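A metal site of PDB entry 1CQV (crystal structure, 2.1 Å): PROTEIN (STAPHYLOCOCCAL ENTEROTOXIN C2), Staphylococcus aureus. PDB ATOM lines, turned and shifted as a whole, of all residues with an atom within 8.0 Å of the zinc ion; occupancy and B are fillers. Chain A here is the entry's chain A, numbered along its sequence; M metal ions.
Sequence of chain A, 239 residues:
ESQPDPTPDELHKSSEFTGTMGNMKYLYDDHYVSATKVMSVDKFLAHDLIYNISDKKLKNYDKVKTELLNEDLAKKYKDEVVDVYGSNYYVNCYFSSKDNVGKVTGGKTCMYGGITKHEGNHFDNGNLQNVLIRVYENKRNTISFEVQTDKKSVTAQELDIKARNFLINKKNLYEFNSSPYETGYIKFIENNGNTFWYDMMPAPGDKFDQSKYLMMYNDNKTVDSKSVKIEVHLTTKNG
The side-chain carboxylate of Asp 83 is in hydrogen-bond range of the backbone NH of Lys 37, at 3.2 Å.
The backbone NH (N) of Asp 83 is in hydrogen-bond range of the backbone carbonyl oxygen (O) of Thr 116.
A ring nitrogen (ND1) of His 122 sits at hydrogen-bond distance from the backbone carbonyl oxygen (O) of Asp 150.
A ring nitrogen (NE2) of His 118 sits close to the side-chain carboxylate (OE1) of Glu 119 (3.3 Å).
The backbone carbonyl oxygen (O) of Val 81 lies within hydrogen-bond range of the backbone NH (N) of His 118 (3.2 Å).
The side-chain carboxylate (OD2) of Asp 83 is bound to the zinc ion.
The zinc ion is bound by NE2 of His 122 (2.2 Å).
A ring nitrogen (ND1) of His 118 binds the zinc ion (2.3 Å).
The zinc ion has three donor atoms within binding distance.
Slightly farther from the zinc ion lies the side-chain carboxylate (OD1) of Asp 83 (2.7 Å).
The nearest printed residue that does not touch the zinc ion is Thr 36 (4.9 Å).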
ATOM      1  N   ALA A  35      -7.619  -9.407   6.783  1.00  0.00           N
ATOM      2  CA  ALA A  35      -6.931 -10.694   6.688  1.00  0.00           C
ATOM      3  C   ALA A  35      -7.840 -11.743   6.094  1.00  0.00           C
ATOM      4  O   ALA A  35      -9.067 -11.637   6.117  1.00  0.00           O
ATOM      5  CB  ALA A  35      -6.355 -11.125   8.035  1.00  0.00           C
ATOM      6  N   THR A  36      -7.242 -12.752   5.449  1.00  0.00           N
ATOM      7  CA  THR A  36      -7.985 -13.852   4.876  1.00  0.00           C
ATOM      8  C   THR A  36      -7.487 -15.205   5.349  1.00  0.00           C
ATOM      9  O   THR A  36      -6.366 -15.519   5.685  1.00  0.00           O
ATOM     10  CB  THR A  36      -8.252 -13.796   3.365  1.00  0.00           C
ATOM     11  OG1 THR A  36      -7.835 -14.951   2.616  1.00  0.00           O
ATOM     12  CG2 THR A  36      -7.845 -12.574   2.636  1.00  0.00           C
ATOM     13  N   LYS A  37      -8.499 -15.984   5.665  1.00  0.00           N
ATOM     14  CA  LYS A  37      -8.420 -17.363   6.140  1.00  0.00           C
ATOM     15  C   LYS A  37      -7.525 -17.489   7.350  1.00  0.00           C
ATOM     16  O   LYS A  37      -6.617 -18.314   7.255  1.00  0.00           O
ATOM     17  CB  LYS A  37      -7.900 -18.224   4.975  1.00  0.00           C
ATOM     18  CG  LYS A  37      -9.023 -18.287   3.921  1.00  0.00           C
ATOM     19  CD  LYS A  37      -8.536 -18.935   2.637  1.00  0.00           C
ATOM     20  CE  LYS A  37      -8.276 -20.427   2.824  1.00  0.00           C
ATOM     21  NZ  LYS A  37      -7.691 -20.969   1.538  1.00  0.00           N
ATOM     22  N   VAL A  38      -7.722 -16.806   8.434  1.00  0.00           N
ATOM     23  CA  VAL A  38      -6.883 -16.920   9.630  1.00  0.00           C
ATOM     24  C   VAL A  38      -7.729 -17.589  10.717  1.00  0.00           C
ATOM     25  O   VAL A  38      -8.963 -17.553  10.691  1.00  0.00           O
ATOM     26  CB  VAL A  38      -6.348 -15.577  10.160  1.00  0.00           C
ATOM     27  CG1 VAL A  38      -5.320 -14.981   9.195  1.00  0.00           C
ATOM     28  CG2 VAL A  38      -7.537 -14.639  10.346  1.00  0.00           C
ATOM     29  N   VAL A  81     -12.070 -20.847  10.471  1.00  0.00           N
ATOM     30  CA  VAL A  81     -11.269 -20.127   9.483  1.00  0.00           C
ATOM     31  C   VAL A  81     -12.078 -18.895   9.050  1.00  0.00           C
ATOM     32  O   VAL A  81     -13.160 -19.032   8.497  1.00  0.00           O
ATOM     33  CB  VAL A  81     -10.976 -21.016   8.245  1.00  0.00           C
ATOM     34  CG1 VAL A  81     -10.182 -20.240   7.197  1.00  0.00           C
ATOM     35  CG2 VAL A  81     -10.309 -22.338   8.654  1.00  0.00           C
ATOM     36  N   VAL A  82     -11.635 -17.659   9.320  1.00  0.00           N
ATOM     37  CA  VAL A  82     -12.401 -16.431   9.167  1.00  0.00           C
ATOM     38  C   VAL A  82     -11.643 -15.400   8.307  1.00  0.00           C
ATOM     39  O   VAL A  82     -10.438 -15.538   8.131  1.00  0.00           O
ATOM     40  CB  VAL A  82     -12.751 -15.804  10.555  1.00  0.00           C
ATOM     41  CG1 VAL A  82     -13.406 -16.808  11.521  1.00  0.00           C
ATOM     42  CG2 VAL A  82     -11.541 -15.147  11.249  1.00  0.00           C
ATOM     43  N   ASP A  83     -12.365 -14.424   7.776  1.00  0.00           N
ATOM     44  CA  ASP A  83     -11.837 -13.230   7.223  1.00  0.00           C
ATOM     45  C   ASP A  83     -12.135 -12.094   8.212  1.00  0.00           C
ATOM     46  O   ASP A  83     -13.073 -12.169   9.010  1.00  0.00           O
ATOM     47  CB  ASP A  83     -12.432 -12.861   5.881  1.00  0.00           C
ATOM     48  CG  ASP A  83     -12.324 -14.001   4.881  1.00  0.00           C
ATOM     49  OD1 ASP A  83     -11.323 -14.746   4.678  1.00  0.00           O
ATOM     50  OD2 ASP A  83     -13.362 -14.181   4.198  1.00  0.00           O
ATOM     51  N   VAL A  84     -11.238 -11.115   8.252  1.00  0.00           N
ATOM     52  CA  VAL A  84     -11.198 -10.042   9.198  1.00  0.00           C
ATOM     53  C   VAL A  84     -11.211  -8.697   8.450  1.00  0.00           C
ATOM     54  O   VAL A  84     -10.449  -8.536   7.500  1.00  0.00           O
ATOM     55  CB  VAL A  84      -9.963 -10.137  10.110  1.00  0.00           C
ATOM     56  CG1 VAL A  84      -9.918  -9.030  11.133  1.00  0.00           C
ATOM     57  CG2 VAL A  84      -9.937 -11.469  10.874  1.00  0.00           C
ATOM     58  N   THR A 116     -15.749 -12.615   9.829  1.00  0.00           N
ATOM     59  CA  THR A 116     -16.748 -13.459   9.127  1.00  0.00           C
ATOM     60  C   THR A 116     -16.210 -14.809   8.695  1.00  0.00           C
ATOM     61  O   THR A 116     -15.080 -14.925   8.185  1.00  0.00           O
ATOM     62  CB  THR A 116     -17.343 -12.782   7.864  1.00  0.00           C
ATOM     63  OG1 THR A 116     -16.229 -12.228   7.135  1.00  0.00           O
ATOM     64  CG2 THR A 116     -18.275 -11.611   8.136  1.00  0.00           C
ATOM     65  N   LYS A 117     -17.030 -15.851   8.776  1.00  0.00           N
ATOM     66  CA  LYS A 117     -16.569 -17.165   8.279  1.00  0.00           C
ATOM     67  C   LYS A 117     -16.135 -17.007   6.814  1.00  0.00           C
ATOM     68  O   LYS A 117     -16.829 -16.421   6.010  1.00  0.00           O
ATOM     69  CB  LYS A 117     -17.562 -18.293   8.358  1.00  0.00           C
ATOM     70  CG  LYS A 117     -18.337 -18.593   9.610  1.00  0.00           C
ATOM     71  CD  LYS A 117     -19.846 -18.860   9.321  1.00  0.00           C
ATOM     72  CE  LYS A 117     -20.693 -18.950  10.593  1.00  0.00           C
ATOM     73  NZ  LYS A 117     -22.163 -19.117  10.327  1.00  0.00           N
ATOM     74  N   HIS A 118     -15.066 -17.625   6.416  1.00  0.00           N
ATOM     75  CA  HIS A 118     -14.629 -17.569   5.011  1.00  0.00           C
ATOM     76  C   HIS A 118     -15.489 -18.504   4.162  1.00  0.00           C
ATOM     77  O   HIS A 118     -15.991 -18.138   3.089  1.00  0.00           O
ATOM     78  CB  HIS A 118     -13.177 -18.032   5.023  1.00  0.00           C
ATOM     79  CG  HIS A 118     -12.724 -18.550   3.691  1.00  0.00           C
ATOM     80  ND1 HIS A 118     -12.520 -17.661   2.676  1.00  0.00           N
ATOM     81  CD2 HIS A 118     -12.407 -19.781   3.209  1.00  0.00           C
ATOM     82  CE1 HIS A 118     -12.095 -18.268   1.585  1.00  0.00           C
ATOM     83  NE2 HIS A 118     -12.037 -19.552   1.895  1.00  0.00           N
ATOM     84  N   GLU A 119     -15.626 -19.758   4.624  1.00  0.00           N
ATOM     85  CA  GLU A 119     -16.240 -20.749   3.749  1.00  0.00           C
ATOM     86  C   GLU A 119     -17.677 -20.420   3.446  1.00  0.00           C
ATOM     87  O   GLU A 119     -18.395 -19.956   4.335  1.00  0.00           O
ATOM     88  CB  GLU A 119     -16.299 -22.150   4.402  1.00  0.00           C
ATOM     89  CG  GLU A 119     -16.059 -23.213   3.281  1.00  0.00           C
ATOM     90  CD  GLU A 119     -14.536 -23.075   2.927  1.00  0.00           C
ATOM     91  OE1 GLU A 119     -14.077 -22.157   2.166  1.00  0.00           O
ATOM     92  OE2 GLU A 119     -13.748 -23.810   3.363  1.00  0.00           O
ATOM     93  N   GLY A 120     -18.095 -20.561   2.195  1.00  0.00           N
ATOM     94  CA  GLY A 120     -19.436 -20.248   1.776  1.00  0.00           C
ATOM     95  C   GLY A 120     -19.772 -18.769   1.684  1.00  0.00           C
ATOM     96  O   GLY A 120     -20.946 -18.432   1.363  1.00  0.00           O
ATOM     97  N   ASN A 121     -18.815 -17.855   1.906  1.00  0.00           N
ATOM     98  CA  ASN A 121     -19.212 -16.447   2.038  1.00  0.00           C
ATOM     99  C   ASN A 121     -18.804 -15.661   0.804  1.00  0.00           C
ATOM    100  O   ASN A 121     -18.718 -14.408   0.909  1.00  0.00           O
ATOM    101  CB  ASN A 121     -18.584 -15.833   3.323  1.00  0.00           C
ATOM    102  CG  ASN A 121     -19.321 -14.564   3.739  1.00  0.00           C
ATOM    103  OD1 ASN A 121     -20.540 -14.508   3.567  1.00  0.00           O
ATOM    104  ND2 ASN A 121     -18.605 -13.530   4.200  1.00  0.00           N
ATOM    105  N   HIS A 122     -18.400 -16.284  -0.325  1.00  0.00           N
ATOM    106  CA  HIS A 122     -18.035 -15.450  -1.473  1.00  0.00           C
ATOM    107  C   HIS A 122     -18.902 -15.754  -2.708  1.00  0.00           C
ATOM    108  O   HIS A 122     -19.603 -16.743  -2.712  1.00  0.00           O
ATOM    109  CB  HIS A 122     -16.562 -15.530  -1.901  1.00  0.00           C
ATOM    110  CG  HIS A 122     -15.675 -15.130  -0.770  1.00  0.00           C
ATOM    111  ND1 HIS A 122     -15.684 -13.820  -0.373  1.00  0.00           N
ATOM    112  CD2 HIS A 122     -14.830 -15.787   0.083  1.00  0.00           C
ATOM    113  CE1 HIS A 122     -14.864 -13.664   0.662  1.00  0.00           C
ATOM    114  NE2 HIS A 122     -14.363 -14.848   0.957  1.00  0.00           N
ATOM    115  N   ASP A 150     -16.086  -8.259  -1.474  1.00  0.00           N
ATOM    116  CA  ASP A 150     -16.088  -9.627  -1.960  1.00  0.00           C
ATOM    117  C   ASP A 150     -16.945 -10.533  -1.074  1.00  0.00           C
ATOM    118  O   ASP A 150     -16.951 -11.738  -1.314  1.00  0.00           O
ATOM    119  CB  ASP A 150     -14.636 -10.115  -2.010  1.00  0.00           C
ATOM    120  CG  ASP A 150     -13.995 -10.228  -0.667  1.00  0.00           C
ATOM    121  OD1 ASP A 150     -14.328  -9.527   0.335  1.00  0.00           O
ATOM    122  OD2 ASP A 150     -13.058 -11.052  -0.485  1.00  0.00           O
ATOM    123  N   LYS A 151     -17.627 -10.035  -0.058  1.00  0.00           N
ATOM    124  CA  LYS A 151     -18.247 -10.912   0.911  1.00  0.00           C
ATOM    125  C   LYS A 151     -19.774 -10.894   0.788  1.00  0.00           C
ATOM    126  O   LYS A 151     -20.374  -9.834   0.614  1.00  0.00           O
ATOM    127  CB  LYS A 151     -17.911 -10.535   2.329  1.00  0.00           C
ATOM    128  CG  LYS A 151     -16.450 -10.713   2.710  1.00  0.00           C
ATOM    129  CD  LYS A 151     -16.318 -10.257   4.168  1.00  0.00           C
ATOM    130  CE  LYS A 151     -14.828 -10.203   4.506  1.00  0.00           C
ATOM    131  NZ  LYS A 151     -14.100  -9.098   3.790  1.00  0.00           N
HETATM  132 ZN    ZN M   1     -12.790 -15.344   2.460  1.00  0.00          ZN
